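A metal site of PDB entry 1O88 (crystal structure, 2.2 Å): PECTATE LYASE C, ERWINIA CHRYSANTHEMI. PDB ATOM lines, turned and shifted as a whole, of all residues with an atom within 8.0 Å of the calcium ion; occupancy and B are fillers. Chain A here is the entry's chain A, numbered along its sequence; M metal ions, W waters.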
ATOM      1  N   TRP A 106     -25.363  22.200 -22.144  1.00  0.00           N
ATOM      2  CA  TRP A 106     -24.500  21.804 -21.030  1.00  0.00           C
ATOM      3  C   TRP A 106     -24.449  22.885 -19.970  1.00  0.00           C
ATOM      4  O   TRP A 106     -23.947  23.975 -20.196  1.00  0.00           O
ATOM      5  CB  TRP A 106     -23.107  21.480 -21.564  1.00  0.00           C
ATOM      6  CG  TRP A 106     -23.153  20.480 -22.703  1.00  0.00           C
ATOM      7  CD1 TRP A 106     -24.023  19.437 -22.835  1.00  0.00           C
ATOM      8  CD2 TRP A 106     -22.304  20.444 -23.866  1.00  0.00           C
ATOM      9  NE1 TRP A 106     -23.779  18.764 -24.006  1.00  0.00           N
ATOM     10  CE2 TRP A 106     -22.738  19.358 -24.653  1.00  0.00           C
ATOM     11  CE3 TRP A 106     -21.240  21.230 -24.308  1.00  0.00           C
ATOM     12  CZ2 TRP A 106     -22.134  19.028 -25.868  1.00  0.00           C
ATOM     13  CZ3 TRP A 106     -20.636  20.907 -25.516  1.00  0.00           C
ATOM     14  CH2 TRP A 106     -21.082  19.799 -26.283  1.00  0.00           C
ATOM     15  N   GLY A 126     -20.658  11.244 -29.486  1.00  0.00           N
ATOM     16  CA  GLY A 126     -20.957  10.424 -28.341  1.00  0.00           C
ATOM     17  C   GLY A 126     -19.689   9.997 -27.631  1.00  0.00           C
ATOM     18  O   GLY A 126     -19.690   9.770 -26.427  1.00  0.00           O
ATOM     19  N   LYS A 128     -17.131  11.872 -27.209  1.00  0.00           N
ATOM     20  CA  LYS A 128     -16.564  13.041 -26.536  1.00  0.00           C
ATOM     21  C   LYS A 128     -17.596  13.794 -25.670  1.00  0.00           C
ATOM     22  O   LYS A 128     -17.647  15.030 -25.653  1.00  0.00           O
ATOM     23  CB  LYS A 128     -15.882  13.987 -27.543  1.00  0.00           C
ATOM     24  CG  LYS A 128     -14.680  13.358 -28.268  1.00  0.00           C
ATOM     25  CD  LYS A 128     -14.135  14.314 -29.321  1.00  0.00           C
ATOM     26  CE  LYS A 128     -13.152  13.631 -30.229  1.00  0.00           C
ATOM     27  NZ  LYS A 128     -13.834  12.791 -31.254  1.00  0.00           N
ATOM     28  N   ASP A 129     -18.407  13.025 -24.966  1.00  0.00           N
ATOM     29  CA  ASP A 129     -19.439  13.533 -24.059  1.00  0.00           C
ATOM     30  C   ASP A 129     -20.490  14.424 -24.702  1.00  0.00           C
ATOM     31  O   ASP A 129     -20.872  15.448 -24.141  1.00  0.00           O
ATOM     32  CB  ASP A 129     -18.771  14.257 -22.867  1.00  0.00           C
ATOM     33  CG  ASP A 129     -19.483  13.978 -21.545  1.00  0.00           C
ATOM     34  OD1 ASP A 129     -20.284  13.022 -21.452  1.00  0.00           O
ATOM     35  OD2 ASP A 129     -19.221  14.729 -20.585  1.00  0.00           O
ATOM     36  N   GLY A 130     -21.003  13.981 -25.835  1.00  0.00           N
ATOM     37  CA  GLY A 130     -22.029  14.733 -26.522  1.00  0.00           C
ATOM     38  C   GLY A 130     -23.411  14.533 -25.929  1.00  0.00           C
ATOM     39  O   GLY A 130     -24.296  14.006 -26.586  1.00  0.00           O
ATOM     40  N   ASP A 131     -23.594  14.939 -24.663  1.00  0.00           N
ATOM     41  CA  ASP A 131     -24.888  14.816 -23.971  1.00  0.00           C
ATOM     42  C   ASP A 131     -25.941  15.748 -24.529  1.00  0.00           C
ATOM     43  O   ASP A 131     -25.622  16.842 -25.006  1.00  0.00           O
ATOM     44  CB  ASP A 131     -24.727  15.162 -22.489  1.00  0.00           C
ATOM     45  CG  ASP A 131     -23.879  14.183 -21.731  1.00  0.00           C
ATOM     46  OD1 ASP A 131     -23.964  12.970 -22.015  1.00  0.00           O
ATOM     47  OD2 ASP A 131     -23.130  14.626 -20.848  1.00  0.00           O
ATOM     48  N   MET A 132     -27.204  15.358 -24.411  1.00  0.00           N
ATOM     49  CA  MET A 132     -28.308  16.179 -24.865  1.00  0.00           C
ATOM     50  C   MET A 132     -28.515  17.276 -23.821  1.00  0.00           C
ATOM     51  O   MET A 132     -28.618  18.446 -24.161  1.00  0.00           O
ATOM     52  CB  MET A 132     -29.569  15.352 -25.076  1.00  0.00           C
ATOM     53  CG  MET A 132     -29.399  14.327 -26.205  1.00  0.00           C
ATOM     54  SD  MET A 132     -30.892  13.497 -26.678  1.00  0.00           S
ATOM     55  CE  MET A 132     -30.539  11.867 -26.158  1.00  0.00           C
ATOM     56  N   ILE A 133     -28.500  16.873 -22.557  1.00  0.00           N
ATOM     57  CA  ILE A 133     -28.612  17.801 -21.443  1.00  0.00           C
ATOM     58  C   ILE A 133     -27.619  17.300 -20.360  1.00  0.00           C
ATOM     59  O   ILE A 133     -27.530  16.108 -20.083  1.00  0.00           O
ATOM     60  CB  ILE A 133     -30.036  17.855 -20.818  1.00  0.00           C
ATOM     61  CG1 ILE A 133     -31.105  18.196 -21.863  1.00  0.00           C
ATOM     62  CG2 ILE A 133     -30.077  18.884 -19.658  1.00  0.00           C
ATOM     63  CD1 ILE A 133     -31.252  19.622 -22.189  1.00  0.00           C
ATOM     64  N   ARG A 134     -26.800  18.216 -19.844  1.00  0.00           N
ATOM     65  CA  ARG A 134     -25.873  17.887 -18.791  1.00  0.00           C
ATOM     66  C   ARG A 134     -26.038  18.931 -17.694  1.00  0.00           C
ATOM     67  O   ARG A 134     -26.107  20.130 -17.977  1.00  0.00           O
ATOM     68  CB  ARG A 134     -24.435  17.867 -19.281  1.00  0.00           C
ATOM     69  CG  ARG A 134     -23.470  17.339 -18.243  1.00  0.00           C
ATOM     70  CD  ARG A 134     -22.148  16.920 -18.857  1.00  0.00           C
ATOM     71  NE  ARG A 134     -21.494  18.024 -19.545  1.00  0.00           N
ATOM     72  CZ  ARG A 134     -21.100  17.978 -20.810  1.00  0.00           C
ATOM     73  NH1 ARG A 134     -21.292  16.892 -21.542  1.00  0.00           N
ATOM     74  NH2 ARG A 134     -20.435  19.005 -21.313  1.00  0.00           N
ATOM     75  N   PHE A 165     -23.746   6.962 -28.805  1.00  0.00           N
ATOM     76  CA  PHE A 165     -24.482   8.165 -28.437  1.00  0.00           C
ATOM     77  C   PHE A 165     -24.278   8.340 -26.954  1.00  0.00           C
ATOM     78  O   PHE A 165     -24.117   7.346 -26.225  1.00  0.00           O
ATOM     79  CB  PHE A 165     -25.989   8.024 -28.727  1.00  0.00           C
ATOM     80  CG  PHE A 165     -26.353   8.144 -30.183  1.00  0.00           C
ATOM     81  CD1 PHE A 165     -26.132   9.330 -30.880  1.00  0.00           C
ATOM     82  CD2 PHE A 165     -26.899   7.062 -30.871  1.00  0.00           C
ATOM     83  CE1 PHE A 165     -26.428   9.431 -32.231  1.00  0.00           C
ATOM     84  CE2 PHE A 165     -27.201   7.150 -32.224  1.00  0.00           C
ATOM     85  CZ  PHE A 165     -26.959   8.340 -32.909  1.00  0.00           C
ATOM     86  N   GLU A 166     -24.205   9.584 -26.494  1.00  0.00           N
ATOM     87  CA  GLU A 166     -24.066   9.831 -25.071  1.00  0.00           C
ATOM     88  C   GLU A 166     -25.461   9.885 -24.429  1.00  0.00           C
ATOM     89  O   GLU A 166     -26.438   9.440 -25.033  1.00  0.00           O
ATOM     90  CB  GLU A 166     -23.247  11.098 -24.795  1.00  0.00           C
ATOM     91  CG  GLU A 166     -21.891  10.788 -24.137  1.00  0.00           C
ATOM     92  CD  GLU A 166     -22.007  10.038 -22.798  1.00  0.00           C
ATOM     93  OE1 GLU A 166     -22.523  10.601 -21.801  1.00  0.00           O
ATOM     94  OE2 GLU A 166     -21.571   8.880 -22.727  1.00  0.00           O
ATOM     95  N   SER A 167     -25.569  10.526 -23.275  1.00  0.00           N
ATOM     96  CA  SER A 167     -26.832  10.561 -22.524  1.00  0.00           C
ATOM     97  C   SER A 167     -27.884  11.630 -22.811  1.00  0.00           C
ATOM     98  O   SER A 167     -27.604  12.649 -23.441  1.00  0.00           O
ATOM     99  CB  SER A 167     -26.500  10.565 -21.050  1.00  0.00           C
ATOM    100  OG  SER A 167     -25.487   9.606 -20.788  1.00  0.00           O
ATOM    101  N   ALA A 168     -29.108  11.377 -22.351  1.00  0.00           N
ATOM    102  CA  ALA A 168     -30.215  12.305 -22.532  1.00  0.00           C
ATOM    103  C   ALA A 168     -30.135  13.378 -21.463  1.00  0.00           C
ATOM    104  O   ALA A 168     -30.218  14.566 -21.777  1.00  0.00           O
ATOM    105  CB  ALA A 168     -31.555  11.575 -22.439  1.00  0.00           C
ATOM    106  N   VAL A 169     -30.006  12.968 -20.199  1.00  0.00           N
ATOM    107  CA  VAL A 169     -29.878  13.917 -19.090  1.00  0.00           C
ATOM    108  C   VAL A 169     -28.909  13.437 -18.014  1.00  0.00           C
ATOM    109  O   VAL A 169     -29.309  12.740 -17.077  1.00  0.00           O
ATOM    110  CB  VAL A 169     -31.255  14.262 -18.394  1.00  0.00           C
ATOM    111  CG1 VAL A 169     -31.071  15.419 -17.414  1.00  0.00           C
ATOM    112  CG2 VAL A 169     -32.322  14.656 -19.436  1.00  0.00           C
ATOM    113  N   ASP A 170     -27.639  13.822 -18.127  1.00  0.00           N
ATOM    114  CA  ASP A 170     -26.632  13.449 -17.138  1.00  0.00           C
ATOM    115  C   ASP A 170     -26.529  14.510 -16.055  1.00  0.00           C
ATOM    116  O   ASP A 170     -26.348  15.688 -16.358  1.00  0.00           O
ATOM    117  CB  ASP A 170     -25.270  13.287 -17.788  1.00  0.00           C
ATOM    118  CG  ASP A 170     -25.039  11.891 -18.306  1.00  0.00           C
ATOM    119  OD1 ASP A 170     -25.871  11.007 -18.034  1.00  0.00           O
ATOM    120  OD2 ASP A 170     -24.015  11.688 -18.979  1.00  0.00           O
ATOM    121  N   ILE A 171     -26.625  14.076 -14.810  1.00  0.00           N
ATOM    122  CA  ILE A 171     -26.529  14.987 -13.666  1.00  0.00           C
ATOM    123  C   ILE A 171     -25.330  14.572 -12.834  1.00  0.00           C
ATOM    124  O   ILE A 171     -25.128  13.386 -12.583  1.00  0.00           O
ATOM    125  CB  ILE A 171     -27.808  14.911 -12.783  1.00  0.00           C
ATOM    126  CG1 ILE A 171     -29.025  15.376 -13.582  1.00  0.00           C
ATOM    127  CG2 ILE A 171     -27.609  15.734 -11.507  1.00  0.00           C
ATOM    128  CD1 ILE A 171     -30.392  15.010 -12.979  1.00  0.00           C
ATOM    129  N   LYS A 172     -24.496  15.527 -12.452  1.00  0.00           N
ATOM    130  CA  LYS A 172     -23.321  15.217 -11.652  1.00  0.00           C
ATOM    131  C   LYS A 172     -22.878  16.377 -10.810  1.00  0.00           C
ATOM    132  O   LYS A 172     -23.329  17.505 -10.991  1.00  0.00           O
ATOM    133  CB  LYS A 172     -22.166  14.762 -12.518  1.00  0.00           C
ATOM    134  CG  LYS A 172     -21.764  15.719 -13.595  1.00  0.00           C
ATOM    135  CD  LYS A 172     -20.365  15.355 -14.048  1.00  0.00           C
ATOM    136  CE  LYS A 172     -20.094  15.773 -15.462  1.00  0.00           C
ATOM    137  NZ  LYS A 172     -18.692  15.403 -15.799  1.00  0.00           N
ATOM    138  N   LYS A 190     -28.206   5.135 -22.944  1.00  0.00           N
ATOM    139  CA  LYS A 190     -27.822   5.564 -21.597  1.00  0.00           C
ATOM    140  C   LYS A 190     -28.605   6.810 -21.302  1.00  0.00           C
ATOM    141  O   LYS A 190     -28.229   7.902 -21.746  1.00  0.00           O
ATOM    142  CB  LYS A 190     -26.321   5.866 -21.589  1.00  0.00           C
ATOM    143  CG  LYS A 190     -25.471   4.652 -21.939  1.00  0.00           C
ATOM    144  CD  LYS A 190     -24.353   5.007 -22.893  1.00  0.00           C
ATOM    145  CE  LYS A 190     -23.443   6.049 -22.298  1.00  0.00           C
ATOM    146  NZ  LYS A 190     -22.209   6.173 -23.106  1.00  0.00           N
ATOM    147  N   GLY A 192     -29.439   8.554 -18.224  1.00  0.00           N
ATOM    148  CA  GLY A 192     -28.899   9.588 -17.381  1.00  0.00           C
ATOM    149  C   GLY A 192     -28.285   9.168 -16.079  1.00  0.00           C
ATOM    150  O   GLY A 192     -28.818   8.313 -15.372  1.00  0.00           O
ATOM    151  N   LEU A 193     -27.161   9.802 -15.746  1.00  0.00           N
ATOM    152  CA  LEU A 193     -26.436   9.557 -14.522  1.00  0.00           C
ATOM    153  C   LEU A 193     -26.973  10.458 -13.449  1.00  0.00           C
ATOM    154  O   LEU A 193     -27.493  11.541 -13.730  1.00  0.00           O
ATOM    155  CB  LEU A 193     -24.970   9.949 -14.712  1.00  0.00           C
ATOM    156  CG  LEU A 193     -24.138   9.113 -15.649  1.00  0.00           C
ATOM    157  CD1 LEU A 193     -22.777   9.754 -15.794  1.00  0.00           C
ATOM    158  CD2 LEU A 193     -24.009   7.710 -15.084  1.00  0.00           C
ATOM    159  N   ARG A 218     -30.155   3.171 -17.063  1.00  0.00           N
ATOM    160  CA  ARG A 218     -29.916   4.385 -16.286  1.00  0.00           C
ATOM    161  C   ARG A 218     -31.118   5.320 -16.203  1.00  0.00           C
ATOM    162  O   ARG A 218     -31.107   6.411 -16.821  1.00  0.00           O
ATOM    163  CB  ARG A 218     -28.710   5.137 -16.839  1.00  0.00           C
ATOM    164  CG  ARG A 218     -27.455   4.307 -16.992  1.00  0.00           C
ATOM    165  CD  ARG A 218     -26.300   5.202 -17.393  1.00  0.00           C
ATOM    166  NE  ARG A 218     -25.088   4.434 -17.609  1.00  0.00           N
ATOM    167  CZ  ARG A 218     -23.907   4.972 -17.943  1.00  0.00           C
ATOM    168  NH1 ARG A 218     -23.785   6.296 -18.099  1.00  0.00           N
ATOM    169  NH2 ARG A 218     -22.842   4.205 -18.071  1.00  0.00           N
HETATM  170 CA    CA M   1     -22.227  12.316 -20.349  1.00  0.00          CA
HETATM  171  O   HOH W   1     -21.430  13.678 -18.514  1.00  0.00           O
HETATM  172  O   HOH W   2     -20.825  10.444 -19.311  1.00  0.00           O
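Four residues have an atom within 4 Å of the calcium ion: Asp 129, Asp 131, Glu 166 and Asp 170.
The nearest printed residue that does not touch the calcium ion is Ser 167 (4.3 Å).
The side-chain carboxylate (OD2) of Asp 131 sits close to the guanidinium group (NH1) of Arg 134.
OD1 of Asp 170 sits at hydrogen-bond distance from N of Leu 193 (2.9 Å).
The backbone carbonyl oxygen of Ile 133 sits at hydrogen-bond distance from the backbone NH of Asp 170, 3.0 Å away.
The backbone carbonyl oxygen (O) of Asp 131 is in hydrogen-bond range of the indole nitrogen (NE1) of Trp 106 (2.8 Å).
The side-chain carboxylate of Glu 166 sits close to the side-chain hydroxyl of Ser 167 (3.3 Å).
The side-chain carboxylate (OD2) of Asp 129 is in salt-bridge range of the guanidinium group (NH1) of Arg 134.
NZ of Lys 190 is in salt-bridge range of OE2 of Glu 166.
The side-chain carboxylate (OD1) of Asp 131 sits close to the backbone NH (N) of Ser 167 (3.2 Å).
The calcium ion is bound by OE1 of Glu 166 (2.3 Å).
OD2 of Asp 170 binds the calcium ion (2.3 Å).
OD1 of Asp 129 is bound to the calcium ion (2.3 Å).
Water W1 is bound to the calcium ion (2.4 Å).
The calcium ion is bound by the side-chain carboxylate (OD1) of Asp 131 (2.5 Å).
The calcium ion is bound by OD2 of Asp 131.
Water W2 binds the calcium ion, at 2.6 Å.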
